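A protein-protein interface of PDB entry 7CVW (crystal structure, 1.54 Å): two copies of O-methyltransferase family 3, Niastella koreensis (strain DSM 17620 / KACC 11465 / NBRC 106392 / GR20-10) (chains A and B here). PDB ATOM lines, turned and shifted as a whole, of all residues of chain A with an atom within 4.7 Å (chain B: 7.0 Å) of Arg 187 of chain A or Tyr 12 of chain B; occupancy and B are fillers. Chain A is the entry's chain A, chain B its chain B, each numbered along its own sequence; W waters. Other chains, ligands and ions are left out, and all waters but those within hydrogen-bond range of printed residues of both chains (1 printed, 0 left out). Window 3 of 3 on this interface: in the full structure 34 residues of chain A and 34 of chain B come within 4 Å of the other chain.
Arg 187 of chain A touches one residue of chain B.
Printed residues of chain B within 4 Å of Leu 174 of chain A: Ser 8, Val 9 and Tyr 12.
Of the printed residues of chain A, Val 9 of chain B touches Ile 168 (3.8 Å) and Leu 174 (3.96 Å).
Printed residues of chain B within 4 Å of Val 173 of chain A: Tyr 12 (3.7 Å).
Of the printed residues of chain A, Leu 16 of chain B touches Asn 190.
Ile 13 of chain B touches none of the printed residues of chain A.
Ala 191 of chain A touches none of the printed residues of chain B.
The nearest residue of chain B that does not touch Arg 187 of chain A is Leu 16 of chain B (6.2 Å).
The nearest printed residue of chain B that does not touch Leu 174 of chain A is Ile 13 of chain B (6.4 Å).
O of Val 173 of chain A is in hydrogen-bond range of NH1 of Arg 187 of chain A, 2.7 Å away.
O of Ala 186 of chain A lies close to ND2 of Asn 190 of chain A, 3.3 Å away.
OH of Tyr 12 of chain B sits at hydrogen-bond distance from ND2 of Asn 190 of chain A (3.2 Å).
No position is printed for both chains.
Water W1 bridges OH of Tyr 12 of chain B (2.6 Å) and O of Arg 187 of chain A (2.8 Å).
Hydrophobic or aromatic side chains of chain A that line the printed part of chain B: Ile 168, Val 173 and Leu 174.
Of the 13 printed residues of chain B, 4 touch a printed residue of chain A.
Hydrophobic or aromatic side chains of chain B within 4 Å of the printed part of chain A: Val 9, Tyr 12 and Leu 16.
Among the printed residues, no Asp or Glu carboxylate lies within 4 Å of a Lys or Arg side-chain nitrogen of the other chain.
Among the printed residues, pairs that only touch across the chains: Ile 168 of chain A with Val 9 of chain B, Val 173 of chain A with Tyr 12 of chain B, Leu 174 of chain A with Ser 8 of chain B, Leu 174 of chain A with Val 9 of chain B, Leu 174 of chain A with Tyr 12 of chain B, Arg 187 of chain A with Tyr 12 of chain B and Asn 190 of chain A with Leu 16 of chain B.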
ATOM      1  N   ILE A 168      11.425  22.569   7.123  1.00  0.00           N
ATOM      2  CA  ILE A 168      10.561  22.453   5.906  1.00  0.00           C
ATOM      3  C   ILE A 168      11.262  21.662   4.791  1.00  0.00           C
ATOM      4  O   ILE A 168      10.581  20.896   4.098  1.00  0.00           O
ATOM      5  CB  ILE A 168      10.080  23.845   5.440  1.00  0.00           C
ATOM      6  CG1 ILE A 168       9.109  24.461   6.452  1.00  0.00           C
ATOM      7  CG2 ILE A 168       9.454  23.788   4.058  1.00  0.00           C
ATOM      8  CD1 ILE A 168       7.896  23.614   6.790  1.00  0.00           C
ATOM      9  N   VAL A 173       8.870  17.719   3.830  1.00  0.00           N
ATOM     10  CA  VAL A 173       8.144  17.336   5.071  1.00  0.00           C
ATOM     11  C   VAL A 173       6.701  16.929   4.717  1.00  0.00           C
ATOM     12  O   VAL A 173       6.049  16.355   5.590  1.00  0.00           O
ATOM     13  CB  VAL A 173       8.157  18.420   6.164  1.00  0.00           C
ATOM     14  CG1 VAL A 173       9.544  18.594   6.759  1.00  0.00           C
ATOM     15  CG2 VAL A 173       7.578  19.731   5.646  1.00  0.00           C
ATOM     16  N   LEU A 174       6.187  17.281   3.536  1.00  0.00           N
ATOM     17  CA  LEU A 174       4.823  16.844   3.121  1.00  0.00           C
ATOM     18  C   LEU A 174       4.817  15.344   2.793  1.00  0.00           C
ATOM     19  O   LEU A 174       3.740  14.743   2.749  1.00  0.00           O
ATOM     20  CB  LEU A 174       4.380  17.648   1.903  1.00  0.00           C
ATOM     21  CG  LEU A 174       4.133  19.133   2.142  1.00  0.00           C
ATOM     22  CD1 LEU A 174       3.513  19.742   0.909  1.00  0.00           C
ATOM     23  CD2 LEU A 174       3.231  19.357   3.346  1.00  0.00           C
ATOM     24  N   ASP A 175       5.969  14.745   2.534  1.00  0.00           N
ATOM     25  CA  ASP A 175       6.074  13.316   2.132  1.00  0.00           C
ATOM     26  C   ASP A 175       6.175  12.440   3.385  1.00  0.00           C
ATOM     27  O   ASP A 175       7.294  12.292   3.948  1.00  0.00           O
ATOM     28  CB  ASP A 175       7.273  13.095   1.208  1.00  0.00           C
ATOM     29  CG  ASP A 175       7.433  11.656   0.732  1.00  0.00           C
ATOM     30  OD1 ASP A 175       6.604  10.797   1.106  1.00  0.00           O
ATOM     31  OD2 ASP A 175       8.385  11.419  -0.003  1.00  0.00           O
ATOM     32  N   GLU A 176       5.055  11.837   3.782  1.00  0.00           N
ATOM     33  CA  GLU A 176       4.966  10.936   4.963  1.00  0.00           C
ATOM     34  C   GLU A 176       5.889   9.731   4.767  1.00  0.00           C
ATOM     35  O   GLU A 176       6.293   9.155   5.767  1.00  0.00           O
ATOM     36  CB  GLU A 176       3.521  10.472   5.201  1.00  0.00           C
ATOM     37  CG  GLU A 176       2.742  10.193   3.929  1.00  0.00           C
ATOM     38  CD  GLU A 176       2.110  11.422   3.291  1.00  0.00           C
ATOM     39  OE1 GLU A 176       1.172  11.972   3.905  1.00  0.00           O
ATOM     40  OE2 GLU A 176       2.559  11.842   2.193  1.00  0.00           O
ATOM     41  N   VAL A 183      14.543  14.852   6.987  1.00  0.00           N
ATOM     42  CA  VAL A 183      13.112  15.148   6.695  1.00  0.00           C
ATOM     43  C   VAL A 183      12.277  14.453   7.767  1.00  0.00           C
ATOM     44  O   VAL A 183      11.342  15.060   8.295  1.00  0.00           O
ATOM     45  CB  VAL A 183      12.728  14.722   5.270  1.00  0.00           C
ATOM     46  CG1 VAL A 183      11.232  14.853   5.023  1.00  0.00           C
ATOM     47  CG2 VAL A 183      13.510  15.509   4.235  1.00  0.00           C
ATOM     48  N   GLN A 184      12.593  13.205   8.101  1.00  0.00           N
ATOM     49  CA  GLN A 184      11.882  12.507   9.195  1.00  0.00           C
ATOM     50  C   GLN A 184      12.068  13.281  10.507  1.00  0.00           C
ATOM     51  O   GLN A 184      11.085  13.425  11.290  1.00  0.00           O
ATOM     52  CB  GLN A 184      12.392  11.080   9.362  1.00  0.00           C
ATOM     53  CG  GLN A 184      12.177  10.211   8.142  1.00  0.00           C
ATOM     54  CD  GLN A 184      12.638   8.793   8.384  1.00  0.00           C
ATOM     55  OE1 GLN A 184      13.267   8.477   9.393  1.00  0.00           O
ATOM     56  NE2 GLN A 184      12.310   7.915   7.455  1.00  0.00           N
ATOM     57  N   GLY A 185      13.273  13.776  10.765  1.00  0.00           N
ATOM     58  CA  GLY A 185      13.532  14.535  11.999  1.00  0.00           C
ATOM     59  C   GLY A 185      12.677  15.780  12.052  1.00  0.00           C
ATOM     60  O   GLY A 185      12.110  16.082  13.112  1.00  0.00           O
ATOM     61  N   ALA A 186      12.570  16.482  10.935  1.00  0.00           N
ATOM     62  CA  ALA A 186      11.758  17.713  10.852  1.00  0.00           C
ATOM     63  C   ALA A 186      10.279  17.374  11.052  1.00  0.00           C
ATOM     64  O   ALA A 186       9.613  18.089  11.774  1.00  0.00           O
ATOM     65  CB  ALA A 186      12.008  18.386   9.526  1.00  0.00           C
ATOM     66  N   ARG A 187       9.769  16.342  10.371  1.00  0.00           N
ATOM     67  CA  ARG A 187       8.338  15.956  10.459  1.00  0.00           C
ATOM     68  C   ARG A 187       8.002  15.623  11.901  1.00  0.00           C
ATOM     69  O   ARG A 187       6.934  15.995  12.359  1.00  0.00           O
ATOM     70  CB  ARG A 187       7.974  14.768   9.569  1.00  0.00           C
ATOM     71  CG  ARG A 187       7.865  15.120   8.090  1.00  0.00           C
ATOM     72  CD  ARG A 187       7.602  13.890   7.214  1.00  0.00           C
ATOM     73  NE  ARG A 187       6.529  13.078   7.778  1.00  0.00           N
ATOM     74  CZ  ARG A 187       5.230  13.351   7.710  1.00  0.00           C
ATOM     75  NH1 ARG A 187       4.774  14.403   7.045  1.00  0.00           N
ATOM     76  NH2 ARG A 187       4.365  12.550   8.306  1.00  0.00           N
ATOM     77  N   ARG A 188       8.862  14.883  12.591  1.00  0.00           N
ATOM     78  CA  ARG A 188       8.567  14.411  13.959  1.00  0.00           C
ATOM     79  C   ARG A 188       8.570  15.619  14.898  1.00  0.00           C
ATOM     80  O   ARG A 188       7.695  15.724  15.753  1.00  0.00           O
ATOM     81  CB  ARG A 188       9.564  13.330  14.380  1.00  0.00           C
ATOM     82  CG  ARG A 188       9.181  12.640  15.674  1.00  0.00           C
ATOM     83  CD  ARG A 188       9.933  11.343  15.879  1.00  0.00           C
ATOM     84  NE  ARG A 188      11.341  11.599  16.111  1.00  0.00           N
ATOM     85  CZ  ARG A 188      11.877  11.852  17.305  1.00  0.00           C
ATOM     86  NH1 ARG A 188      11.151  11.786  18.416  1.00  0.00           N
ATOM     87  NH2 ARG A 188      13.172  12.127  17.381  1.00  0.00           N
ATOM     88  N   PHE A 189       9.549  16.520  14.743  1.00  0.00           N
ATOM     89  CA  PHE A 189       9.636  17.765  15.537  1.00  0.00           C
ATOM     90  C   PHE A 189       8.372  18.598  15.304  1.00  0.00           C
ATOM     91  O   PHE A 189       7.846  19.191  16.235  1.00  0.00           O
ATOM     92  CB  PHE A 189      10.913  18.525  15.157  1.00  0.00           C
ATOM     93  CG  PHE A 189      10.964  19.910  15.730  1.00  0.00           C
ATOM     94  CD1 PHE A 189      11.411  20.112  17.021  1.00  0.00           C
ATOM     95  CD2 PHE A 189      10.508  21.001  14.992  1.00  0.00           C
ATOM     96  CE1 PHE A 189      11.438  21.386  17.559  1.00  0.00           C
ATOM     97  CE2 PHE A 189      10.521  22.270  15.548  1.00  0.00           C
ATOM     98  CZ  PHE A 189      10.996  22.456  16.817  1.00  0.00           C
ATOM     99  N   ASN A 190       7.954  18.745  14.055  1.00  0.00           N
ATOM    100  CA  ASN A 190       6.788  19.610  13.708  1.00  0.00           C
ATOM    101  C   ASN A 190       5.530  19.014  14.349  1.00  0.00           C
ATOM    102  O   ASN A 190       4.674  19.773  14.877  1.00  0.00           O
ATOM    103  CB  ASN A 190       6.651  19.766  12.194  1.00  0.00           C
ATOM    104  CG  ASN A 190       7.750  20.605  11.573  1.00  0.00           C
ATOM    105  OD1 ASN A 190       8.482  21.298  12.284  1.00  0.00           O
ATOM    106  ND2 ASN A 190       7.893  20.495  10.262  1.00  0.00           N
ATOM    107  N   ALA A 191       5.373  17.696  14.279  1.00  0.00           N
ATOM    108  CA  ALA A 191       4.234  17.001  14.938  1.00  0.00           C
ATOM    109  C   ALA A 191       4.255  17.268  16.445  1.00  0.00           C
ATOM    110  O   ALA A 191       3.197  17.523  17.036  1.00  0.00           O
ATOM    111  CB  ALA A 191       4.265  15.521  14.660  1.00  0.00           C
ATOM    112  N   GLU B   7       1.670  26.792  -1.031  1.00  0.00           N
ATOM    113  CA  GLU B   7       0.282  26.714  -0.512  1.00  0.00           C
ATOM    114  C   GLU B   7       0.115  25.421   0.286  1.00  0.00           C
ATOM    115  O   GLU B   7      -0.418  25.467   1.388  1.00  0.00           O
ATOM    116  CB  GLU B   7      -0.748  26.745  -1.638  1.00  0.00           C
ATOM    117  CG  GLU B   7      -0.733  28.039  -2.423  1.00  0.00           C
ATOM    118  CD  GLU B   7      -1.858  28.187  -3.437  1.00  0.00           C
ATOM    119  OE1 GLU B   7      -2.873  27.460  -3.314  1.00  0.00           O
ATOM    120  OE2 GLU B   7      -1.723  29.058  -4.337  1.00  0.00           O
ATOM    121  N   SER B   8       0.586  24.293  -0.252  1.00  0.00           N
ATOM    122  CA  SER B   8       0.481  22.984   0.437  1.00  0.00           C
ATOM    123  C   SER B   8       1.239  23.022   1.768  1.00  0.00           C
ATOM    124  O   SER B   8       0.727  22.526   2.779  1.00  0.00           O
ATOM    125  CB  SER B   8       0.977  21.892  -0.445  1.00  0.00           C
ATOM    126  OG  SER B   8       0.096  21.746  -1.551  1.00  0.00           O
ATOM    127  N   VAL B   9       2.436  23.586   1.758  1.00  0.00           N
ATOM    128  CA  VAL B   9       3.242  23.662   3.004  1.00  0.00           C
ATOM    129  C   VAL B   9       2.540  24.611   3.976  1.00  0.00           C
ATOM    130  O   VAL B   9       2.539  24.336   5.183  1.00  0.00           O
ATOM    131  CB  VAL B   9       4.690  24.089   2.715  1.00  0.00           C
ATOM    132  CG1 VAL B   9       5.414  24.432   4.011  1.00  0.00           C
ATOM    133  CG2 VAL B   9       5.463  23.030   1.928  1.00  0.00           C
ATOM    134  N   ASP B  10       1.933  25.708   3.507  1.00  0.00           N
ATOM    135  CA  ASP B  10       1.232  26.625   4.450  1.00  0.00           C
ATOM    136  C   ASP B  10       0.073  25.871   5.136  1.00  0.00           C
ATOM    137  O   ASP B  10      -0.122  26.032   6.341  1.00  0.00           O
ATOM    138  CB  ASP B  10       0.696  27.883   3.762  1.00  0.00           C
ATOM    139  CG  ASP B  10       1.084  29.196   4.441  1.00  0.00           C
ATOM    140  OD1 ASP B  10       2.040  29.188   5.232  1.00  0.00           O
ATOM    141  OD2 ASP B  10       0.481  30.227   4.107  1.00  0.00           O
ATOM    142  N   HIS B  11      -0.684  25.051   4.401  1.00  0.00           N
ATOM    143  CA  HIS B  11      -1.815  24.261   4.958  1.00  0.00           C
ATOM    144  C   HIS B  11      -1.290  23.261   6.000  1.00  0.00           C
ATOM    145  O   HIS B  11      -1.900  23.118   7.061  1.00  0.00           O
ATOM    146  CB  HIS B  11      -2.573  23.575   3.810  1.00  0.00           C
ATOM    147  CG  HIS B  11      -3.339  24.509   2.932  1.00  0.00           C
ATOM    148  ND1 HIS B  11      -3.717  24.158   1.640  1.00  0.00           N
ATOM    149  CD2 HIS B  11      -3.805  25.757   3.136  1.00  0.00           C
ATOM    150  CE1 HIS B  11      -4.375  25.168   1.087  1.00  0.00           C
ATOM    151  NE2 HIS B  11      -4.469  26.153   1.994  1.00  0.00           N
ATOM    152  N   TYR B  12      -0.156  22.624   5.694  1.00  0.00           N
ATOM    153  CA  TYR B  12       0.534  21.702   6.621  1.00  0.00           C
ATOM    154  C   TYR B  12       0.837  22.469   7.906  1.00  0.00           C
ATOM    155  O   TYR B  12       0.531  22.025   9.029  1.00  0.00           O
ATOM    156  CB  TYR B  12       1.760  21.122   5.929  1.00  0.00           C
ATOM    157  CG  TYR B  12       2.772  20.447   6.817  1.00  0.00           C
ATOM    158  CD1 TYR B  12       2.629  19.120   7.195  1.00  0.00           C
ATOM    159  CD2 TYR B  12       3.886  21.128   7.262  1.00  0.00           C
ATOM    160  CE1 TYR B  12       3.589  18.489   7.985  1.00  0.00           C
ATOM    161  CE2 TYR B  12       4.866  20.512   8.022  1.00  0.00           C
ATOM    162  CZ  TYR B  12       4.700  19.198   8.427  1.00  0.00           C
ATOM    163  OH  TYR B  12       5.645  18.562   9.171  1.00  0.00           O
ATOM    164  N   ILE B  13       1.411  23.657   7.768  1.00  0.00           N
ATOM    165  CA  ILE B  13       1.771  24.463   8.975  1.00  0.00           C
ATOM    166  C   ILE B  13       0.510  24.893   9.736  1.00  0.00           C
ATOM    167  O   ILE B  13       0.523  24.854  10.963  1.00  0.00           O
ATOM    168  CB  ILE B  13       2.640  25.675   8.600  1.00  0.00           C
ATOM    169  CG1 ILE B  13       3.996  25.241   8.043  1.00  0.00           C
ATOM    170  CG2 ILE B  13       2.819  26.588   9.797  1.00  0.00           C
ATOM    171  CD1 ILE B  13       4.791  26.337   7.418  1.00  0.00           C
ATOM    172  N   SER B  14      -0.516  25.393   9.058  1.00  0.00           N
ATOM    173  CA  SER B  14      -1.683  25.937   9.777  1.00  0.00           C
ATOM    174  C   SER B  14      -2.477  24.774  10.396  1.00  0.00           C
ATOM    175  O   SER B  14      -3.065  24.980  11.455  1.00  0.00           O
ATOM    176  CB  SER B  14      -2.509  26.848   8.897  1.00  0.00           C
ATOM    177  OG  SER B  14      -2.969  26.189   7.745  1.00  0.00           O
ATOM    178  N   ASP B  15      -2.441  23.581   9.798  1.00  0.00           N
ATOM    179  CA  ASP B  15      -3.048  22.348  10.392  1.00  0.00           C
ATOM    180  C   ASP B  15      -2.411  22.049  11.753  1.00  0.00           C
ATOM    181  O   ASP B  15      -3.112  21.583  12.663  1.00  0.00           O
ATOM    182  CB  ASP B  15      -2.927  21.155   9.449  1.00  0.00           C
ATOM    183  CG  ASP B  15      -3.972  21.161   8.345  1.00  0.00           C
ATOM    184  OD1 ASP B  15      -4.917  21.985   8.422  1.00  0.00           O
ATOM    185  OD2 ASP B  15      -3.842  20.319   7.436  1.00  0.00           O
ATOM    186  N   LEU B  16      -1.109  22.323  11.897  1.00  0.00           N
ATOM    187  CA  LEU B  16      -0.364  22.083  13.159  1.00  0.00           C
ATOM    188  C   LEU B  16      -0.507  23.274  14.121  1.00  0.00           C
ATOM    189  O   LEU B  16      -0.661  23.021  15.343  1.00  0.00           O
ATOM    190  CB  LEU B  16       1.116  21.856  12.811  1.00  0.00           C
ATOM    191  CG  LEU B  16       1.468  20.562  12.094  1.00  0.00           C
ATOM    192  CD1 LEU B  16       2.892  20.581  11.532  1.00  0.00           C
ATOM    193  CD2 LEU B  16       1.317  19.378  13.034  1.00  0.00           C
ATOM    194  N   LEU B  17      -0.367  24.513  13.617  1.00  0.00           N
ATOM    195  CA  LEU B  17      -0.031  25.707  14.444  1.00  0.00           C
ATOM    196  C   LEU B  17      -0.831  26.958  14.046  1.00  0.00           C
ATOM    197  O   LEU B  17      -0.476  28.063  14.557  1.00  0.00           O
ATOM    198  CB  LEU B  17       1.478  25.987  14.339  1.00  0.00           C
ATOM    199  CG  LEU B  17       2.393  24.914  14.936  1.00  0.00           C
ATOM    200  CD1 LEU B  17       3.826  25.177  14.493  1.00  0.00           C
ATOM    201  CD2 LEU B  17       2.270  24.875  16.458  1.00  0.00           C
ATOM    202  N   GLY B  18      -1.832  26.826  13.177  1.00  0.00           N
ATOM    203  CA  GLY B  18      -2.568  27.990  12.647  1.00  0.00           C
ATOM    204  C   GLY B  18      -4.058  27.846  12.781  1.00  0.00           C
ATOM    205  O   GLY B  18      -4.750  28.338  11.922  1.00  0.00           O
ATOM    206  N   ASN B  44      -1.093  31.874   9.150  1.00  0.00           N
ATOM    207  CA  ASN B  44       0.261  31.636   9.730  1.00  0.00           C
ATOM    208  C   ASN B  44       0.954  32.991   9.941  1.00  0.00           C
ATOM    209  O   ASN B  44       1.693  33.143  10.933  1.00  0.00           O
ATOM    210  CB  ASN B  44       1.088  30.682   8.888  1.00  0.00           C
ATOM    211  CG  ASN B  44       0.551  29.269   8.898  1.00  0.00           C
ATOM    212  OD1 ASN B  44      -0.030  28.836   9.886  1.00  0.00           O
ATOM    213  ND2 ASN B  44       0.755  28.563   7.802  1.00  0.00           N
HETATM  214  O   HOH W   1       4.902  16.476  10.537  1.00  0.00           O
